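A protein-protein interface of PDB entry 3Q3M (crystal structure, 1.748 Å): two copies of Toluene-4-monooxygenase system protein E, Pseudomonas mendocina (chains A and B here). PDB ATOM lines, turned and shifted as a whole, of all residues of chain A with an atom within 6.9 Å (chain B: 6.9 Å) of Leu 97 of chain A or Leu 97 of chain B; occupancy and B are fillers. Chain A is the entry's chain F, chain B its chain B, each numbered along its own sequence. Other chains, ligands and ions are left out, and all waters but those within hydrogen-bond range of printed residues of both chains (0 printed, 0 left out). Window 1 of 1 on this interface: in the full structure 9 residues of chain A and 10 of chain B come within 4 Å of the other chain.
OG of Ser 96 of chain B lies within hydrogen-bond range of O of Ser 92 of chain B (3.2 Å). The backbone carbonyl oxygen (O) of Ser 92 of chain A sits at hydrogen-bond distance from the side-chain hydroxyl (OG) of Ser 96 of chain A, at 3.0 Å.
Among the printed residues, merely in contact across the chains: Tyr 93 of chain A with Ser 96 of chain B (3.3 Å), Ser 96 of chain A with Tyr 93 of chain B (3.4 Å), Tyr 93 of chain A with Tyr 93 of chain B (3.9 Å), Tyr 93 of chain A with Gln 100 of chain B (3.9 Å), Tyr 93 of chain A with Leu 97 of chain B (3.9 Å), Phe 101 of chain A with Leu 249 of chain B (3.97 Å), Leu 249 of chain A with Phe 101 of chain B (3.98 Å), Leu 97 of chain A with Leu 97 of chain B (3.99 Å), Leu 97 of chain A with Tyr 93 of chain B (3.99 Å) and Gln 100 of chain A with Tyr 93 of chain B (3.99 Å).
Of the printed residues of chain B, Leu 97 of chain A touches Tyr 93 and Leu 97. Of the printed residues of chain A, Leu 97 of chain B touches Tyr 93 (3.9 Å) and Leu 97 (3.99 Å). Of the printed residues of chain A, Leu 249 of chain B touches Phe 101 (3.97 Å). Printed residues of chain B within 4 Å of Leu 249 of chain A: Phe 101 (3.98 Å). Gln 95 of chain B touches none of the printed residues of chain A. Ser 253 of chain B touches none of the printed residues of chain A. The nearest printed residue of chain B that does not touch Leu 97 of chain A is Leu 249 of chain B (5.3 Å).
Printed residues of chain B that touch a printed residue of chain A: Tyr 93, Ser 96, Leu 97, Gln 100, Phe 101 and Leu 249. Among the printed residues, 10 pairs touch across the chains.
Tyr 93 of chain A touches its own counterpart, Tyr 93 of chain B. Tyr 93 of chain A touches Ser 96 of chain B, and with the chains exchanged Ser 96 of chain A touches Tyr 93 of chain B. Tyr 93 of chain A touches Leu 97 of chain B, and with the chains exchanged Leu 97 of chain A touches Tyr 93 of chain B. Tyr 93 of chain A touches Gln 100 of chain B, and with the chains exchanged Gln 100 of chain A touches Tyr 93 of chain B. Positions printed for both chains: 91, 92, 93, 94, 95, 96, 97, 98, 99, 100, 101, 102, 103, 246, 249, 250 and 253. Of the 10 pairs that touch across the chains among the printed residues, 10 have their exchanged pair printed and touching as well.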
ATOM      1  N   GLU A  91      -2.621  10.987  19.293  1.00  0.00           N
ATOM      2  CA  GLU A  91      -2.605   9.612  19.786  1.00  0.00           C
ATOM      3  C   GLU A  91      -3.853   8.837  19.328  1.00  0.00           C
ATOM      4  O   GLU A  91      -3.777   7.651  19.012  1.00  0.00           O
ATOM      5  CB  GLU A  91      -2.420   9.584  21.299  1.00  0.00           C
ATOM      6  CG  GLU A  91      -2.131   8.208  21.859  1.00  0.00           C
ATOM      7  CD  GLU A  91      -0.841   7.586  21.341  1.00  0.00           C
ATOM      8  OE1 GLU A  91      -0.038   8.226  20.621  1.00  0.00           O
ATOM      9  OE2 GLU A  91      -0.622   6.398  21.648  1.00  0.00           O
ATOM     10  N   SER A  92      -4.999   9.500  19.273  1.00  0.00           N
ATOM     11  CA  SER A  92      -6.194   8.834  18.767  1.00  0.00           C
ATOM     12  C   SER A  92      -6.016   8.486  17.290  1.00  0.00           C
ATOM     13  O   SER A  92      -6.516   7.457  16.819  1.00  0.00           O
ATOM     14  CB  SER A  92      -7.421   9.728  18.952  1.00  0.00           C
ATOM     15  OG  SER A  92      -7.766   9.810  20.319  1.00  0.00           O
ATOM     16  N   TYR A  93      -5.319   9.363  16.565  1.00  0.00           N
ATOM     17  CA  TYR A  93      -4.934   9.091  15.170  1.00  0.00           C
ATOM     18  C   TYR A  93      -4.018   7.863  15.060  1.00  0.00           C
ATOM     19  O   TYR A  93      -4.257   6.975  14.241  1.00  0.00           O
ATOM     20  CB  TYR A  93      -4.286  10.333  14.536  1.00  0.00           C
ATOM     21  CG  TYR A  93      -3.400  10.103  13.303  1.00  0.00           C
ATOM     22  CD1 TYR A  93      -3.949   9.858  12.042  1.00  0.00           C
ATOM     23  CD2 TYR A  93      -2.025  10.195  13.405  1.00  0.00           C
ATOM     24  CE1 TYR A  93      -3.123   9.676  10.905  1.00  0.00           C
ATOM     25  CE2 TYR A  93      -1.186  10.014  12.299  1.00  0.00           C
ATOM     26  CZ  TYR A  93      -1.737   9.756  11.052  1.00  0.00           C
ATOM     27  OH  TYR A  93      -0.894   9.576   9.967  1.00  0.00           O
ATOM     28  N   VAL A  94      -2.985   7.803  15.892  1.00  0.00           N
ATOM     29  CA  VAL A  94      -2.083   6.650  15.866  1.00  0.00           C
ATOM     30  C   VAL A  94      -2.791   5.359  16.256  1.00  0.00           C
ATOM     31  O   VAL A  94      -2.593   4.336  15.627  1.00  0.00           O
ATOM     32  CB  VAL A  94      -0.882   6.875  16.804  1.00  0.00           C
ATOM     33  CG1 VAL A  94      -0.175   5.548  17.096  1.00  0.00           C
ATOM     34  CG2 VAL A  94       0.065   7.914  16.163  1.00  0.00           C
ATOM     35  N   GLN A  95      -3.611   5.407  17.299  1.00  0.00           N
ATOM     36  CA  GLN A  95      -4.372   4.218  17.704  1.00  0.00           C
ATOM     37  C   GLN A  95      -5.335   3.781  16.580  1.00  0.00           C
ATOM     38  O   GLN A  95      -5.554   2.579  16.371  1.00  0.00           O
ATOM     39  CB  GLN A  95      -5.102   4.464  19.032  1.00  0.00           C
ATOM     40  CG  GLN A  95      -4.141   4.841  20.191  1.00  0.00           C
ATOM     41  CD  GLN A  95      -3.249   3.674  20.631  1.00  0.00           C
ATOM     42  OE1 GLN A  95      -3.734   2.559  20.842  1.00  0.00           O
ATOM     43  NE2 GLN A  95      -1.942   3.930  20.776  1.00  0.00           N
ATOM     44  N   SER A  96      -5.886   4.742  15.839  1.00  0.00           N
ATOM     45  CA  SER A  96      -6.750   4.404  14.710  1.00  0.00           C
ATOM     46  C   SER A  96      -5.969   3.765  13.585  1.00  0.00           C
ATOM     47  O   SER A  96      -6.476   2.833  12.914  1.00  0.00           O
ATOM     48  CB  SER A  96      -7.542   5.629  14.207  1.00  0.00           C
ATOM     49  OG  SER A  96      -8.539   5.968  15.158  1.00  0.00           O
ATOM     50  N   LEU A  97      -4.743   4.247  13.369  1.00  0.00           N
ATOM     51  CA  LEU A  97      -3.862   3.600  12.395  1.00  0.00           C
ATOM     52  C   LEU A  97      -3.610   2.143  12.838  1.00  0.00           C
ATOM     53  O   LEU A  97      -3.714   1.232  12.039  1.00  0.00           O
ATOM     54  CB  LEU A  97      -2.524   4.337  12.274  1.00  0.00           C
ATOM     55  CG  LEU A  97      -2.464   5.654  11.488  1.00  0.00           C
ATOM     56  CD1 LEU A  97      -1.084   6.317  11.703  1.00  0.00           C
ATOM     57  CD2 LEU A  97      -2.731   5.463  10.002  1.00  0.00           C
ATOM     58  N   PHE A  98      -3.311   1.931  14.120  1.00  0.00           N
ATOM     59  CA  PHE A  98      -3.028   0.563  14.612  1.00  0.00           C
ATOM     60  C   PHE A  98      -4.245  -0.332  14.325  1.00  0.00           C
ATOM     61  O   PHE A  98      -4.119  -1.432  13.790  1.00  0.00           O
ATOM     62  CB  PHE A  98      -2.741   0.567  16.118  1.00  0.00           C
ATOM     63  CG  PHE A  98      -1.391   1.161  16.493  1.00  0.00           C
ATOM     64  CD1 PHE A  98      -1.086   1.416  17.814  1.00  0.00           C
ATOM     65  CD2 PHE A  98      -0.427   1.428  15.523  1.00  0.00           C
ATOM     66  CE1 PHE A  98       0.159   1.932  18.185  1.00  0.00           C
ATOM     67  CE2 PHE A  98       0.816   1.965  15.889  1.00  0.00           C
ATOM     68  CZ  PHE A  98       1.099   2.209  17.219  1.00  0.00           C
ATOM     69  N   ASP A  99      -5.428   0.174  14.638  1.00  0.00           N
ATOM     70  CA  ASP A  99      -6.651  -0.613  14.470  1.00  0.00           C
ATOM     71  C   ASP A  99      -6.858  -1.011  12.998  1.00  0.00           C
ATOM     72  O   ASP A  99      -7.109  -2.185  12.678  1.00  0.00           O
ATOM     73  CB  ASP A  99      -7.834   0.202  15.001  1.00  0.00           C
ATOM     74  CG  ASP A  99      -9.129  -0.602  15.119  1.00  0.00           C
ATOM     75  OD1 ASP A  99      -9.116  -1.859  15.105  1.00  0.00           O
ATOM     76  OD2 ASP A  99     -10.183   0.050  15.251  1.00  0.00           O
ATOM     77  N   GLN A 100      -6.764  -0.029  12.102  1.00  0.00           N
ATOM     78  CA  GLN A 100      -7.054  -0.258  10.686  1.00  0.00           C
ATOM     79  C   GLN A 100      -5.976  -1.087   9.992  1.00  0.00           C
ATOM     80  O   GLN A 100      -6.300  -1.934   9.165  1.00  0.00           O
ATOM     81  CB  GLN A 100      -7.277   1.071   9.935  1.00  0.00           C
ATOM     82  CG  GLN A 100      -7.785   0.881   8.479  1.00  0.00           C
ATOM     83  CD  GLN A 100      -8.981  -0.058   8.379  1.00  0.00           C
ATOM     84  OE1 GLN A 100      -9.008  -0.955   7.526  1.00  0.00           O
ATOM     85  NE2 GLN A 100      -9.968   0.127   9.253  1.00  0.00           N
ATOM     86  N   PHE A 101      -4.703  -0.855  10.324  1.00  0.00           N
ATOM     87  CA  PHE A 101      -3.635  -1.647   9.720  1.00  0.00           C
ATOM     88  C   PHE A 101      -3.700  -3.089  10.202  1.00  0.00           C
ATOM     89  O   PHE A 101      -3.422  -4.020   9.439  1.00  0.00           O
ATOM     90  CB  PHE A 101      -2.269  -0.986   9.962  1.00  0.00           C
ATOM     91  CG  PHE A 101      -1.971   0.135   8.992  1.00  0.00           C
ATOM     92  CD1 PHE A 101      -0.962   0.016   8.046  1.00  0.00           C
ATOM     93  CD2 PHE A 101      -2.733   1.292   8.992  1.00  0.00           C
ATOM     94  CE1 PHE A 101      -0.703   1.055   7.134  1.00  0.00           C
ATOM     95  CE2 PHE A 101      -2.493   2.324   8.062  1.00  0.00           C
ATOM     96  CZ  PHE A 101      -1.474   2.194   7.138  1.00  0.00           C
ATOM     97  N   ASN A 102      -4.139  -3.282  11.446  1.00  0.00           N
ATOM     98  CA  ASN A 102      -4.374  -4.643  11.951  1.00  0.00           C
ATOM     99  C   ASN A 102      -5.540  -5.330  11.221  1.00  0.00           C
ATOM    100  O   ASN A 102      -5.448  -6.514  10.866  1.00  0.00           O
ATOM    101  CB  ASN A 102      -4.581  -4.626  13.465  1.00  0.00           C
ATOM    102  CG  ASN A 102      -5.110  -5.921  13.993  1.00  0.00           C
ATOM    103  OD1 ASN A 102      -6.312  -6.182  13.916  1.00  0.00           O
ATOM    104  ND2 ASN A 102      -4.219  -6.765  14.536  1.00  0.00           N
ATOM    105  N   GLU A 103      -6.622  -4.589  10.981  1.00  0.00           N
ATOM    106  CA  GLU A 103      -7.768  -5.131  10.246  1.00  0.00           C
ATOM    107  C   GLU A 103      -7.348  -5.604   8.868  1.00  0.00           C
ATOM    108  O   GLU A 103      -7.862  -6.610   8.359  1.00  0.00           O
ATOM    109  CB  GLU A 103      -8.872  -4.088  10.085  1.00  0.00           C
ATOM    110  CG  GLU A 103      -9.674  -3.830  11.351  1.00  0.00           C
ATOM    111  CD  GLU A 103     -10.460  -5.043  11.805  1.00  0.00           C
ATOM    112  OE1 GLU A 103     -10.255  -5.498  12.961  1.00  0.00           O
ATOM    113  OE2 GLU A 103     -11.282  -5.540  11.000  1.00  0.00           O
ATOM    114  N   LEU A 246       3.122   0.960   7.858  1.00  0.00           N
ATOM    115  CA  LEU A 246       2.709   1.522   9.143  1.00  0.00           C
ATOM    116  C   LEU A 246       3.843   2.272   9.864  1.00  0.00           C
ATOM    117  O   LEU A 246       3.631   3.372  10.361  1.00  0.00           O
ATOM    118  CB  LEU A 246       2.159   0.424  10.057  1.00  0.00           C
ATOM    119  CG  LEU A 246       1.744   0.817  11.485  1.00  0.00           C
ATOM    120  CD1 LEU A 246       0.670   1.892  11.492  1.00  0.00           C
ATOM    121  CD2 LEU A 246       1.212  -0.426  12.178  1.00  0.00           C
ATOM    122  N   LEU A 249       4.419   5.976   9.082  1.00  0.00           N
ATOM    123  CA  LEU A 249       3.385   6.875   9.621  1.00  0.00           C
ATOM    124  C   LEU A 249       3.500   7.061  11.141  1.00  0.00           C
ATOM    125  O   LEU A 249       3.306   8.170  11.662  1.00  0.00           O
ATOM    126  CB  LEU A 249       1.986   6.353   9.257  1.00  0.00           C
ATOM    127  CG  LEU A 249       1.644   6.342   7.755  1.00  0.00           C
ATOM    128  CD1 LEU A 249       0.344   5.570   7.537  1.00  0.00           C
ATOM    129  CD2 LEU A 249       1.492   7.742   7.193  1.00  0.00           C
ATOM    130  N   LEU A 250       3.780   5.970  11.849  1.00  0.00           N
ATOM    131  CA  LEU A 250       3.991   6.023  13.304  1.00  0.00           C
ATOM    132  C   LEU A 250       5.151   6.970  13.607  1.00  0.00           C
ATOM    133  O   LEU A 250       5.061   7.854  14.460  1.00  0.00           O
ATOM    134  CB  LEU A 250       4.348   4.634  13.845  1.00  0.00           C
ATOM    135  CG  LEU A 250       4.679   4.571  15.340  1.00  0.00           C
ATOM    136  CD1 LEU A 250       3.527   5.163  16.169  1.00  0.00           C
ATOM    137  CD2 LEU A 250       4.990   3.130  15.778  1.00  0.00           C
ATOM    138  N   SER A 253       4.498  10.625  13.340  1.00  0.00           N
ATOM    139  CA  SER A 253       3.856  11.183  14.535  1.00  0.00           C
ATOM    140  C   SER A 253       4.873  11.440  15.663  1.00  0.00           C
ATOM    141  O   SER A 253       4.859  12.500  16.329  1.00  0.00           O
ATOM    142  CB  SER A 253       2.714  10.262  15.026  1.00  0.00           C
ATOM    143  OG  SER A 253       2.071  10.805  16.155  1.00  0.00           O
ATOM    144  N   GLU B  91     -13.513  11.067  12.209  1.00  0.00           N
ATOM    145  CA  GLU B  91     -13.266  12.183  11.311  1.00  0.00           C
ATOM    146  C   GLU B  91     -11.940  12.900  11.625  1.00  0.00           C
ATOM    147  O   GLU B  91     -11.233  13.321  10.708  1.00  0.00           O
ATOM    148  CB  GLU B  91     -14.480  13.133  11.279  1.00  0.00           C
ATOM    149  CG  GLU B  91     -14.399  14.185  10.206  1.00  0.00           C
ATOM    150  CD  GLU B  91     -14.457  13.631   8.787  1.00  0.00           C
ATOM    151  OE1 GLU B  91     -14.728  12.423   8.589  1.00  0.00           O
ATOM    152  OE2 GLU B  91     -14.235  14.419   7.846  1.00  0.00           O
ATOM    153  N   SER B  92     -11.603  13.014  12.912  1.00  0.00           N
ATOM    154  CA  SER B  92     -10.296  13.541  13.296  1.00  0.00           C
ATOM    155  C   SER B  92      -9.226  12.705  12.626  1.00  0.00           C
ATOM    156  O   SER B  92      -8.274  13.234  12.069  1.00  0.00           O
ATOM    157  CB  SER B  92     -10.104  13.484  14.814  1.00  0.00           C
ATOM    158  OG  SER B  92      -8.976  14.245  15.193  1.00  0.00           O
ATOM    159  N   TYR B  93      -9.410  11.388  12.673  1.00  0.00           N
ATOM    160  CA  TYR B  93      -8.468  10.432  12.080  1.00  0.00           C
ATOM    161  C   TYR B  93      -8.310  10.661  10.570  1.00  0.00           C
ATOM    162  O   TYR B  93      -7.187  10.809  10.065  1.00  0.00           O
ATOM    163  CB  TYR B  93      -8.932   8.994  12.371  1.00  0.00           C
ATOM    164  CG  TYR B  93      -8.385   7.922  11.448  1.00  0.00           C
ATOM    165  CD1 TYR B  93      -7.045   7.537  11.494  1.00  0.00           C
ATOM    166  CD2 TYR B  93      -9.219   7.271  10.544  1.00  0.00           C
ATOM    167  CE1 TYR B  93      -6.556   6.533  10.653  1.00  0.00           C
ATOM    168  CE2 TYR B  93      -8.733   6.267   9.702  1.00  0.00           C
ATOM    169  CZ  TYR B  93      -7.403   5.908   9.760  1.00  0.00           C
ATOM    170  OH  TYR B  93      -6.938   4.916   8.918  1.00  0.00           O
ATOM    171  N   VAL B  94      -9.433  10.744   9.863  1.00  0.00           N
ATOM    172  CA  VAL B  94      -9.399  11.030   8.413  1.00  0.00           C
ATOM    173  C   VAL B  94      -8.738  12.385   8.106  1.00  0.00           C
ATOM    174  O   VAL B  94      -7.889  12.506   7.198  1.00  0.00           O
ATOM    175  CB  VAL B  94     -10.823  10.954   7.821  1.00  0.00           C
ATOM    176  CG1 VAL B  94     -10.862  11.518   6.378  1.00  0.00           C
ATOM    177  CG2 VAL B  94     -11.324   9.510   7.854  1.00  0.00           C
ATOM    178  N   GLN B  95      -9.121  13.423   8.846  1.00  0.00           N
ATOM    179  CA  GLN B  95      -8.500  14.745   8.659  1.00  0.00           C
ATOM    180  C   GLN B  95      -6.984  14.698   8.889  1.00  0.00           C
ATOM    181  O   GLN B  95      -6.191  15.328   8.160  1.00  0.00           O
ATOM    182  CB  GLN B  95      -9.181  15.804   9.547  1.00  0.00           C
ATOM    183  CG  GLN B  95     -10.674  16.012   9.220  1.00  0.00           C
ATOM    184  CD  GLN B  95     -10.947  16.631   7.839  1.00  0.00           C
ATOM    185  OE1 GLN B  95     -10.422  17.694   7.514  1.00  0.00           O
ATOM    186  NE2 GLN B  95     -11.794  15.976   7.043  1.00  0.00           N
ATOM    187  N   SER B  96      -6.565  13.929   9.887  1.00  0.00           N
ATOM    188  CA  SER B  96      -5.135  13.735  10.117  1.00  0.00           C
ATOM    189  C   SER B  96      -4.441  12.990   8.971  1.00  0.00           C
ATOM    190  O   SER B  96      -3.276  13.252   8.687  1.00  0.00           O
ATOM    191  CB  SER B  96      -4.887  12.992  11.429  1.00  0.00           C
ATOM    192  OG  SER B  96      -5.140  13.838  12.539  1.00  0.00           O
ATOM    193  N   LEU B  97      -5.125  12.028   8.360  1.00  0.00           N
ATOM    194  CA  LEU B  97      -4.563  11.321   7.200  1.00  0.00           C
ATOM    195  C   LEU B  97      -4.390  12.309   6.057  1.00  0.00           C
ATOM    196  O   LEU B  97      -3.351  12.337   5.398  1.00  0.00           O
ATOM    197  CB  LEU B  97      -5.499  10.206   6.720  1.00  0.00           C
ATOM    198  CG  LEU B  97      -5.568   8.919   7.538  1.00  0.00           C
ATOM    199  CD1 LEU B  97      -6.724   8.072   7.003  1.00  0.00           C
ATOM    200  CD2 LEU B  97      -4.248   8.133   7.461  1.00  0.00           C
ATOM    201  N   PHE B  98      -5.425  13.096   5.799  1.00  0.00           N
ATOM    202  CA  PHE B  98      -5.343  14.096   4.733  1.00  0.00           C
ATOM    203  C   PHE B  98      -4.092  14.977   4.962  1.00  0.00           C
ATOM    204  O   PHE B  98      -3.308  15.200   4.040  1.00  0.00           O
ATOM    205  CB  PHE B  98      -6.591  14.988   4.714  1.00  0.00           C
ATOM    206  CG  PHE B  98      -7.852  14.317   4.219  1.00  0.00           C
ATOM    207  CD1 PHE B  98      -9.072  14.971   4.360  1.00  0.00           C
ATOM    208  CD2 PHE B  98      -7.827  13.071   3.591  1.00  0.00           C
ATOM    209  CE1 PHE B  98     -10.255  14.380   3.891  1.00  0.00           C
ATOM    210  CE2 PHE B  98      -8.977  12.486   3.137  1.00  0.00           C
ATOM    211  CZ  PHE B  98     -10.202  13.140   3.290  1.00  0.00           C
ATOM    212  N   ASP B  99      -3.919  15.464   6.189  1.00  0.00           N
ATOM    213  CA  ASP B  99      -2.818  16.388   6.541  1.00  0.00           C
ATOM    214  C   ASP B  99      -1.479  15.712   6.268  1.00  0.00           C
ATOM    215  O   ASP B  99      -0.593  16.278   5.604  1.00  0.00           O
ATOM    216  CB  ASP B  99      -2.926  16.765   8.023  1.00  0.00           C
ATOM    217  CG  ASP B  99      -1.947  17.872   8.441  1.00  0.00           C
ATOM    218  OD1 ASP B  99      -1.351  18.532   7.576  1.00  0.00           O
ATOM    219  OD2 ASP B  99      -1.791  18.082   9.660  1.00  0.00           O
ATOM    220  N   GLN B 100      -1.332  14.482   6.767  1.00  0.00           N
ATOM    221  CA  GLN B 100      -0.041  13.807   6.686  1.00  0.00           C
ATOM    222  C   GLN B 100       0.256  13.366   5.259  1.00  0.00           C
ATOM    223  O   GLN B 100       1.373  13.529   4.792  1.00  0.00           O
ATOM    224  CB  GLN B 100       0.042  12.633   7.681  1.00  0.00           C
ATOM    225  CG  GLN B 100       1.422  11.935   7.748  1.00  0.00           C
ATOM    226  CD  GLN B 100       2.576  12.908   8.021  1.00  0.00           C
ATOM    227  OE1 GLN B 100       2.478  13.794   8.868  1.00  0.00           O
ATOM    228  NE2 GLN B 100       3.666  12.755   7.276  1.00  0.00           N
ATOM    229  N   PHE B 101      -0.733  12.805   4.561  1.00  0.00           N
ATOM    230  CA  PHE B 101      -0.501  12.387   3.186  1.00  0.00           C
ATOM    231  C   PHE B 101      -0.183  13.593   2.307  1.00  0.00           C
ATOM    232  O   PHE B 101       0.634  13.516   1.362  1.00  0.00           O
ATOM    233  CB  PHE B 101      -1.692  11.568   2.650  1.00  0.00           C
ATOM    234  CG  PHE B 101      -1.651  10.135   3.079  1.00  0.00           C
ATOM    235  CD1 PHE B 101      -1.458   9.118   2.154  1.00  0.00           C
ATOM    236  CD2 PHE B 101      -1.720   9.803   4.425  1.00  0.00           C
ATOM    237  CE1 PHE B 101      -1.394   7.780   2.572  1.00  0.00           C
ATOM    238  CE2 PHE B 101      -1.644   8.475   4.846  1.00  0.00           C
ATOM    239  CZ  PHE B 101      -1.486   7.465   3.925  1.00  0.00           C
ATOM    240  N   ASN B 102      -0.789  14.723   2.634  1.00  0.00           N
ATOM    241  CA  ASN B 102      -0.475  15.955   1.916  1.00  0.00           C
ATOM    242  C   ASN B 102       0.977  16.400   2.174  1.00  0.00           C
ATOM    243  O   ASN B 102       1.696  16.786   1.251  1.00  0.00           O
ATOM    244  CB  ASN B 102      -1.457  17.078   2.266  1.00  0.00           C
ATOM    245  CG  ASN B 102      -0.991  18.431   1.732  1.00  0.00           C
ATOM    246  OD1 ASN B 102      -0.189  19.114   2.380  1.00  0.00           O
ATOM    247  ND2 ASN B 102      -1.469  18.810   0.525  1.00  0.00           N
ATOM    248  N   GLU B 103       1.406  16.341   3.424  1.00  0.00           N
ATOM    249  CA  GLU B 103       2.794  16.666   3.754  1.00  0.00           C
ATOM    250  C   GLU B 103       3.765  15.816   2.952  1.00  0.00           C
ATOM    251  O   GLU B 103       4.846  16.264   2.547  1.00  0.00           O
ATOM    252  CB  GLU B 103       3.050  16.448   5.249  1.00  0.00           C
ATOM    253  CG  GLU B 103       2.469  17.518   6.149  1.00  0.00           C
ATOM    254  CD  GLU B 103       3.046  18.886   5.866  1.00  0.00           C
ATOM    255  OE1 GLU B 103       2.264  19.841   5.690  1.00  0.00           O
ATOM    256  OE2 GLU B 103       4.285  19.007   5.817  1.00  0.00           O
ATOM    257  N   LEU B 246      -3.926   6.610  -0.163  1.00  0.00           N
ATOM    258  CA  LEU B 246      -4.866   7.377   0.663  1.00  0.00           C
ATOM    259  C   LEU B 246      -6.309   6.922   0.448  1.00  0.00           C
ATOM    260  O   LEU B 246      -7.056   6.706   1.404  1.00  0.00           O
ATOM    261  CB  LEU B 246      -4.761   8.868   0.347  1.00  0.00           C
ATOM    262  CG  LEU B 246      -5.719   9.793   1.120  1.00  0.00           C
ATOM    263  CD1 LEU B 246      -5.666   9.505   2.617  1.00  0.00           C
ATOM    264  CD2 LEU B 246      -5.400  11.260   0.798  1.00  0.00           C
ATOM    265  N   LEU B 249      -7.686   3.936   2.485  1.00  0.00           N
ATOM    266  CA  LEU B 249      -7.869   4.254   3.901  1.00  0.00           C
ATOM    267  C   LEU B 249      -9.120   5.127   4.105  1.00  0.00           C
ATOM    268  O   LEU B 249      -9.895   4.923   5.031  1.00  0.00           O
ATOM    269  CB  LEU B 249      -6.623   4.965   4.439  1.00  0.00           C
ATOM    270  CG  LEU B 249      -5.418   4.047   4.642  1.00  0.00           C
ATOM    271  CD1 LEU B 249      -4.153   4.887   4.907  1.00  0.00           C
ATOM    272  CD2 LEU B 249      -5.665   3.036   5.780  1.00  0.00           C
ATOM    273  N   LEU B 250      -9.312   6.096   3.226  1.00  0.00           N
ATOM    274  CA  LEU B 250     -10.508   6.931   3.289  1.00  0.00           C
ATOM    275  C   LEU B 250     -11.760   6.095   3.106  1.00  0.00           C
ATOM    276  O   LEU B 250     -12.721   6.246   3.867  1.00  0.00           O
ATOM    277  CB  LEU B 250     -10.454   8.028   2.240  1.00  0.00           C
ATOM    278  CG  LEU B 250     -11.720   8.877   2.111  1.00  0.00           C
ATOM    279  CD1 LEU B 250     -11.949   9.670   3.393  1.00  0.00           C
ATOM    280  CD2 LEU B 250     -11.517   9.824   0.899  1.00  0.00           C
ATOM    281  N   SER B 253     -12.799   4.071   6.096  1.00  0.00           N
ATOM    282  CA  SER B 253     -13.575   4.854   7.070  1.00  0.00           C
ATOM    283  C   SER B 253     -15.026   5.043   6.637  1.00  0.00           C
ATOM    284  O   SER B 253     -15.944   4.930   7.452  1.00  0.00           O
ATOM    285  CB  SER B 253     -12.935   6.218   7.350  1.00  0.00           C
ATOM    286  OG  SER B 253     -13.629   6.893   8.391  1.00  0.00           O
